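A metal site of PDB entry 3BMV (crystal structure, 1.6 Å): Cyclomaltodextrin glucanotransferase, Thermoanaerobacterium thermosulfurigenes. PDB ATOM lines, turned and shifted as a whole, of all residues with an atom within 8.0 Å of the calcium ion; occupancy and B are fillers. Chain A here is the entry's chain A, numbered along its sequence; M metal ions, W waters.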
ATOM      1  N   PRO A 139      -6.054  -8.017  16.481  1.00  0.00           N
ATOM      2  CA  PRO A 139      -5.880  -6.746  17.176  1.00  0.00           C
ATOM      3  C   PRO A 139      -6.831  -5.636  16.730  1.00  0.00           C
ATOM      4  O   PRO A 139      -6.743  -4.513  17.242  1.00  0.00           O
ATOM      5  CB  PRO A 139      -4.428  -6.380  16.853  1.00  0.00           C
ATOM      6  CG  PRO A 139      -4.200  -6.951  15.500  1.00  0.00           C
ATOM      7  CD  PRO A 139      -4.987  -8.246  15.479  1.00  0.00           C
ATOM      8  N   ASN A 140      -7.743  -5.938  15.810  1.00  0.00           N
ATOM      9  CA  ASN A 140      -8.707  -4.929  15.364  1.00  0.00           C
ATOM     10  C   ASN A 140      -9.723  -4.524  16.439  1.00  0.00           C
ATOM     11  O   ASN A 140     -10.209  -3.399  16.469  1.00  0.00           O
ATOM     12  CB  ASN A 140      -9.458  -5.380  14.104  1.00  0.00           C
ATOM     13  CG  ASN A 140     -10.420  -4.319  13.608  1.00  0.00           C
ATOM     14  OD1 ASN A 140      -9.993  -3.250  13.144  1.00  0.00           O
ATOM     15  ND2 ASN A 140     -11.716  -4.590  13.690  1.00  0.00           N
ATOM     16  N   HIS A 141     -10.052  -5.480  17.312  1.00  0.00           N
ATOM     17  CA  HIS A 141     -11.190  -5.288  18.201  1.00  0.00           C
ATOM     18  C   HIS A 141     -11.106  -6.193  19.418  1.00  0.00           C
ATOM     19  O   HIS A 141     -10.313  -7.145  19.453  1.00  0.00           O
ATOM     20  CB  HIS A 141     -12.495  -5.604  17.453  1.00  0.00           C
ATOM     21  CG  HIS A 141     -12.484  -6.961  16.815  1.00  0.00           C
ATOM     22  ND1 HIS A 141     -12.226  -7.140  15.474  1.00  0.00           N
ATOM     23  CD2 HIS A 141     -12.641  -8.194  17.344  1.00  0.00           C
ATOM     24  CE1 HIS A 141     -12.241  -8.435  15.200  1.00  0.00           C
ATOM     25  NE2 HIS A 141     -12.492  -9.099  16.321  1.00  0.00           N
ATOM     26  N   HIS A 177     -12.327   3.350  19.182  1.00  0.00           N
ATOM     27  CA  HIS A 177     -12.961   4.316  18.289  1.00  0.00           C
ATOM     28  C   HIS A 177     -14.436   4.469  18.607  1.00  0.00           C
ATOM     29  O   HIS A 177     -15.117   3.497  18.936  1.00  0.00           O
ATOM     30  CB  HIS A 177     -12.834   3.885  16.832  1.00  0.00           C
ATOM     31  CG  HIS A 177     -11.441   3.909  16.304  1.00  0.00           C
ATOM     32  ND1 HIS A 177     -10.895   2.858  15.603  1.00  0.00           N
ATOM     33  CD2 HIS A 177     -10.479   4.855  16.377  1.00  0.00           C
ATOM     34  CE1 HIS A 177      -9.656   3.148  15.277  1.00  0.00           C
ATOM     35  NE2 HIS A 177      -9.373   4.356  15.734  1.00  0.00           N
ATOM     36  N   GLU A 188     -11.280   3.843   4.160  1.00  0.00           N
ATOM     37  CA  GLU A 188     -11.247   4.649   5.392  1.00  0.00           C
ATOM     38  C   GLU A 188     -12.367   4.305   6.358  1.00  0.00           C
ATOM     39  O   GLU A 188     -12.124   4.080   7.556  1.00  0.00           O
ATOM     40  CB  GLU A 188     -11.307   6.144   5.039  1.00  0.00           C
ATOM     41  CG  GLU A 188     -11.373   7.054   6.266  1.00  0.00           C
ATOM     42  CD  GLU A 188     -11.363   8.536   5.941  1.00  0.00           C
ATOM     43  OE1 GLU A 188     -11.340   8.929   4.761  1.00  0.00           O
ATOM     44  OE2 GLU A 188     -11.387   9.318   6.922  1.00  0.00           O
ATOM     45  N   ASP A 189     -13.588   4.263   5.847  1.00  0.00           N
ATOM     46  CA  ASP A 189     -14.758   3.969   6.679  1.00  0.00           C
ATOM     47  C   ASP A 189     -14.567   2.643   7.424  1.00  0.00           C
ATOM     48  O   ASP A 189     -14.881   2.541   8.615  1.00  0.00           O
ATOM     49  CB  ASP A 189     -16.024   3.950   5.815  1.00  0.00           C
ATOM     50  CG  ASP A 189     -17.298   4.045   6.636  1.00  0.00           C
ATOM     51  OD1 ASP A 189     -17.792   5.180   6.858  1.00  0.00           O
ATOM     52  OD2 ASP A 189     -17.784   2.985   7.072  1.00  0.00           O
ATOM     53  N   GLY A 190     -14.030   1.645   6.724  1.00  0.00           N
ATOM     54  CA  GLY A 190     -13.842   0.307   7.286  1.00  0.00           C
ATOM     55  C   GLY A 190     -12.703   0.178   8.283  1.00  0.00           C
ATOM     56  O   GLY A 190     -12.612  -0.831   8.978  1.00  0.00           O
ATOM     57  N   ILE A 191     -11.833   1.172   8.337  1.00  0.00           N
ATOM     58  CA  ILE A 191     -10.710   1.147   9.270  1.00  0.00           C
ATOM     59  C   ILE A 191     -11.058   1.775  10.619  1.00  0.00           C
ATOM     60  O   ILE A 191     -10.718   1.220  11.683  1.00  0.00           O
ATOM     61  CB  ILE A 191      -9.442   1.821   8.665  1.00  0.00           C
ATOM     62  CG1 ILE A 191      -8.861   0.959   7.535  1.00  0.00           C
ATOM     63  CG2 ILE A 191      -8.382   2.054   9.747  1.00  0.00           C
ATOM     64  CD1 ILE A 191      -7.903   1.710   6.622  1.00  0.00           C
ATOM     65  N   TYR A 192     -11.721   2.933  10.593  1.00  0.00           N
ATOM     66  CA  TYR A 192     -11.921   3.753  11.795  1.00  0.00           C
ATOM     67  C   TYR A 192     -13.260   3.524  12.508  1.00  0.00           C
ATOM     68  O   TYR A 192     -13.427   3.960  13.651  1.00  0.00           O
ATOM     69  CB  TYR A 192     -11.664   5.241  11.504  1.00  0.00           C
ATOM     70  CG  TYR A 192     -10.210   5.479  11.164  1.00  0.00           C
ATOM     71  CD1 TYR A 192      -9.271   5.679  12.177  1.00  0.00           C
ATOM     72  CD2 TYR A 192      -9.764   5.443   9.846  1.00  0.00           C
ATOM     73  CE1 TYR A 192      -7.911   5.871  11.875  1.00  0.00           C
ATOM     74  CE2 TYR A 192      -8.414   5.635   9.531  1.00  0.00           C
ATOM     75  CZ  TYR A 192      -7.496   5.834  10.552  1.00  0.00           C
ATOM     76  OH  TYR A 192      -6.170   6.011  10.246  1.00  0.00           O
ATOM     77  N   ARG A 193     -14.180   2.837  11.845  1.00  0.00           N
ATOM     78  CA  ARG A 193     -15.488   2.522  12.427  1.00  0.00           C
ATOM     79  C   ARG A 193     -15.538   1.043  12.810  1.00  0.00           C
ATOM     80  O   ARG A 193     -14.718   0.243  12.350  1.00  0.00           O
ATOM     81  CB  ARG A 193     -16.622   2.890  11.467  1.00  0.00           C
ATOM     82  CG  ARG A 193     -16.579   4.339  10.974  1.00  0.00           C
ATOM     83  CD  ARG A 193     -17.888   4.751  10.313  1.00  0.00           C
ATOM     84  NE  ARG A 193     -17.765   5.969   9.494  1.00  0.00           N
ATOM     85  CZ  ARG A 193     -17.916   7.214   9.953  1.00  0.00           C
ATOM     86  NH1 ARG A 193     -17.797   8.238   9.105  1.00  0.00           N
ATOM     87  NH2 ARG A 193     -18.191   7.452  11.221  1.00  0.00           N
ATOM     88  N   ASN A 194     -16.510   0.673  13.647  1.00  0.00           N
ATOM     89  CA  ASN A 194     -16.627  -0.699  14.145  1.00  0.00           C
ATOM     90  C   ASN A 194     -17.055  -1.695  13.082  1.00  0.00           C
ATOM     91  O   ASN A 194     -17.952  -1.410  12.276  1.00  0.00           O
ATOM     92  CB  ASN A 194     -17.677  -0.785  15.271  1.00  0.00           C
ATOM     93  CG  ASN A 194     -17.343   0.078  16.471  1.00  0.00           C
ATOM     94  OD1 ASN A 194     -16.184   0.424  16.719  1.00  0.00           O
ATOM     95  ND2 ASN A 194     -18.365   0.410  17.257  1.00  0.00           N
ATOM     96  N   LEU A 195     -16.428  -2.875  13.099  1.00  0.00           N
ATOM     97  CA  LEU A 195     -16.925  -4.037  12.377  1.00  0.00           C
ATOM     98  C   LEU A 195     -18.095  -4.595  13.169  1.00  0.00           C
ATOM     99  O   LEU A 195     -17.924  -5.040  14.309  1.00  0.00           O
ATOM    100  CB  LEU A 195     -15.852  -5.110  12.249  1.00  0.00           C
ATOM    101  CG  LEU A 195     -14.659  -4.892  11.342  1.00  0.00           C
ATOM    102  CD1 LEU A 195     -13.732  -6.107  11.397  1.00  0.00           C
ATOM    103  CD2 LEU A 195     -15.119  -4.630   9.910  1.00  0.00           C
ATOM    104  N   LEU A 198     -18.438  -4.888  17.178  1.00  0.00           N
ATOM    105  CA  LEU A 198     -17.174  -5.186  17.838  1.00  0.00           C
ATOM    106  C   LEU A 198     -16.468  -3.883  18.174  1.00  0.00           C
ATOM    107  O   LEU A 198     -16.268  -3.036  17.300  1.00  0.00           O
ATOM    108  CB  LEU A 198     -16.276  -6.049  16.948  1.00  0.00           C
ATOM    109  CG  LEU A 198     -16.849  -7.399  16.514  1.00  0.00           C
ATOM    110  CD1 LEU A 198     -16.017  -7.976  15.370  1.00  0.00           C
ATOM    111  CD2 LEU A 198     -16.910  -8.350  17.685  1.00  0.00           C
ATOM    112  N   ALA A 199     -16.123  -3.716  19.447  1.00  0.00           N
ATOM    113  CA  ALA A 199     -15.447  -2.495  19.918  1.00  0.00           C
ATOM    114  C   ALA A 199     -14.119  -2.315  19.205  1.00  0.00           C
ATOM    115  O   ALA A 199     -13.182  -3.090  19.417  1.00  0.00           O
ATOM    116  CB  ALA A 199     -15.257  -2.549  21.429  1.00  0.00           C
ATOM    117  N   ASP A 200     -14.032  -1.292  18.352  1.00  0.00           N
ATOM    118  CA  ASP A 200     -12.855  -1.098  17.498  1.00  0.00           C
ATOM    119  C   ASP A 200     -11.704  -0.524  18.306  1.00  0.00           C
ATOM    120  O   ASP A 200     -11.816   0.579  18.856  1.00  0.00           O
ATOM    121  CB  ASP A 200     -13.190  -0.171  16.329  1.00  0.00           C
ATOM    122  CG  ASP A 200     -12.329  -0.452  15.105  1.00  0.00           C
ATOM    123  OD1 ASP A 200     -12.272  -1.615  14.652  1.00  0.00           O
ATOM    124  OD2 ASP A 200     -11.703   0.505  14.594  1.00  0.00           O
ATOM    125  N   LEU A 201     -10.606  -1.268  18.394  1.00  0.00           N
ATOM    126  CA  LEU A 201      -9.443  -0.775  19.120  1.00  0.00           C
ATOM    127  C   LEU A 201      -8.790   0.426  18.429  1.00  0.00           C
ATOM    128  O   LEU A 201      -8.731   0.494  17.195  1.00  0.00           O
ATOM    129  CB  LEU A 201      -8.424  -1.902  19.366  1.00  0.00           C
ATOM    130  CG  LEU A 201      -8.789  -2.835  20.523  1.00  0.00           C
ATOM    131  CD1 LEU A 201      -7.986  -4.138  20.445  1.00  0.00           C
ATOM    132  CD2 LEU A 201      -8.590  -2.151  21.882  1.00  0.00           C
ATOM    133  N   ASN A 202      -8.344   1.371  19.234  1.00  0.00           N
ATOM    134  CA  ASN A 202      -7.640   2.529  18.720  1.00  0.00           C
ATOM    135  C   ASN A 202      -6.132   2.299  18.812  1.00  0.00           C
ATOM    136  O   ASN A 202      -5.522   2.633  19.815  1.00  0.00           O
ATOM    137  CB  ASN A 202      -8.043   3.792  19.485  1.00  0.00           C
ATOM    138  CG  ASN A 202      -7.292   5.020  19.016  1.00  0.00           C
ATOM    139  OD1 ASN A 202      -6.611   4.980  17.984  1.00  0.00           O
ATOM    140  ND2 ASN A 202      -7.396   6.114  19.760  1.00  0.00           N
ATOM    141  N   GLN A 203      -5.557   1.723  17.762  1.00  0.00           N
ATOM    142  CA  GLN A 203      -4.131   1.367  17.775  1.00  0.00           C
ATOM    143  C   GLN A 203      -3.215   2.597  17.808  1.00  0.00           C
ATOM    144  O   GLN A 203      -2.032   2.478  18.123  1.00  0.00           O
ATOM    145  CB  GLN A 203      -3.755   0.465  16.593  1.00  0.00           C
ATOM    146  CG  GLN A 203      -4.482  -0.882  16.557  1.00  0.00           C
ATOM    147  CD  GLN A 203      -5.809  -0.810  15.811  1.00  0.00           C
ATOM    148  OE1 GLN A 203      -6.127   0.194  15.173  1.00  0.00           O
ATOM    149  NE2 GLN A 203      -6.585  -1.881  15.878  1.00  0.00           N
ATOM    150  N   ALA A 231      -8.536  -9.362   9.831  1.00  0.00           N
ATOM    151  CA  ALA A 231      -9.157  -8.073   9.483  1.00  0.00           C
ATOM    152  C   ALA A 231      -8.160  -6.978   9.097  1.00  0.00           C
ATOM    153  O   ALA A 231      -8.291  -5.829   9.541  1.00  0.00           O
ATOM    154  CB  ALA A 231     -10.075  -7.598  10.638  1.00  0.00           C
ATOM    155  N   LYS A 233      -7.695  -5.369   6.380  1.00  0.00           N
ATOM    156  CA  LYS A 233      -8.284  -4.250   5.641  1.00  0.00           C
ATOM    157  C   LYS A 233      -8.916  -3.220   6.598  1.00  0.00           C
ATOM    158  O   LYS A 233      -9.272  -2.114   6.176  1.00  0.00           O
ATOM    159  CB  LYS A 233      -9.328  -4.768   4.643  1.00  0.00           C
ATOM    160  CG  LYS A 233      -9.894  -3.689   3.731  1.00  0.00           C
ATOM    161  CD  LYS A 233     -10.899  -4.257   2.753  1.00  0.00           C
ATOM    162  CE  LYS A 233     -11.387  -3.190   1.783  1.00  0.00           C
ATOM    163  NZ  LYS A 233     -12.475  -3.718   0.895  1.00  0.00           N
ATOM    164  N   HIS A 234      -9.046  -3.589   7.864  1.00  0.00           N
ATOM    165  CA  HIS A 234      -9.804  -2.783   8.837  1.00  0.00           C
ATOM    166  C   HIS A 234      -8.940  -2.115   9.912  1.00  0.00           C
ATOM    167  O   HIS A 234      -9.458  -1.557  10.884  1.00  0.00           O
ATOM    168  CB  HIS A 234     -10.917  -3.627   9.433  1.00  0.00           C
ATOM    169  CG  HIS A 234     -11.859  -4.145   8.402  1.00  0.00           C
ATOM    170  ND1 HIS A 234     -12.754  -3.325   7.732  1.00  0.00           N
ATOM    171  CD2 HIS A 234     -12.004  -5.378   7.851  1.00  0.00           C
ATOM    172  CE1 HIS A 234     -13.435  -4.043   6.851  1.00  0.00           C
ATOM    173  NE2 HIS A 234     -12.998  -5.289   6.913  1.00  0.00           N
ATOM    174  N   MET A 235      -7.631  -2.184   9.700  1.00  0.00           N
ATOM    175  CA  MET A 235      -6.656  -1.437  10.503  1.00  0.00           C
ATOM    176  C   MET A 235      -5.780  -0.643   9.557  1.00  0.00           C
ATOM    177  O   MET A 235      -5.639  -1.018   8.392  1.00  0.00           O
ATOM    178  CB  MET A 235      -5.812  -2.385  11.358  1.00  0.00           C
ATOM    179  CG  MET A 235      -6.619  -3.102  12.433  1.00  0.00           C
ATOM    180  SD  MET A 235      -5.687  -4.377  13.305  1.00  0.00           S
ATOM    181  CE  MET A 235      -5.636  -5.655  12.046  1.00  0.00           C
ATOM    182  N   PRO A 236      -5.189   0.475  10.039  1.00  0.00           N
ATOM    183  CA  PRO A 236      -4.347   1.255   9.139  1.00  0.00           C
ATOM    184  C   PRO A 236      -3.159   0.450   8.639  1.00  0.00           C
ATOM    185  O   PRO A 236      -2.542  -0.287   9.421  1.00  0.00           O
ATOM    186  CB  PRO A 236      -3.872   2.409  10.013  1.00  0.00           C
ATOM    187  CG  PRO A 236      -4.926   2.520  11.082  1.00  0.00           C
ATOM    188  CD  PRO A 236      -5.263   1.087  11.375  1.00  0.00           C
HETATM  189 CA    CA M   1     -10.431  -0.874  12.975  1.00  0.00          CA
HETATM  190  O   HOH W   1     -12.492  -1.303  11.718  1.00  0.00           O
HETATM  191  O   HOH W   2      -9.316  -1.311  15.176  1.00  0.00           O
HETATM  192  O   HOH W   3      -8.282   0.408  13.181  1.00  0.00           O
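The backbone carbonyl oxygen of Asp 200 lies within hydrogen-bond range of the backbone NH of His 177 (2.8 Å).
N of Asp 200 lies close to OD1 of Asn 194, at 3.2 Å.
The side-chain sulfur (SD) of Met 235 is in hydrogen-bond range of the backbone NH (N) of Asn 140, 3.6 Å away.
The backbone NH (N) of Leu 201 is in hydrogen-bond range of the backbone carbonyl oxygen (O) of Asn 140, 2.9 Å away.
A ring nitrogen (ND1) of His 141 lies within hydrogen-bond range of the side-chain amide nitrogen (ND2) of Asn 140.
A ring nitrogen (ND1) of His 234 sits at hydrogen-bond distance from the backbone carbonyl oxygen (O) of Gly 190 (2.8 Å).
Of the 23 residues printed, 4 come within 4 Å of the calcium ion.
The calcium ion is bound by the backbone carbonyl oxygen (O) of His 234, the side-chain amide oxygen (OD1) of Asn 140, water W1, the backbone carbonyl oxygen (O) of Ile 191, the side-chain carboxylate (OD2) of Asp 200, water W2, water W3 and the side-chain carboxylate (OD1) of Asp 200.
The calcium ion has eight donor atoms within binding distance.
Water W2 lies within hydrogen-bond range of O of Asn 140 (2.6 Å), O of Leu 201 (2.8 Å) and NE2 of Gln 203 (2.9 Å).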
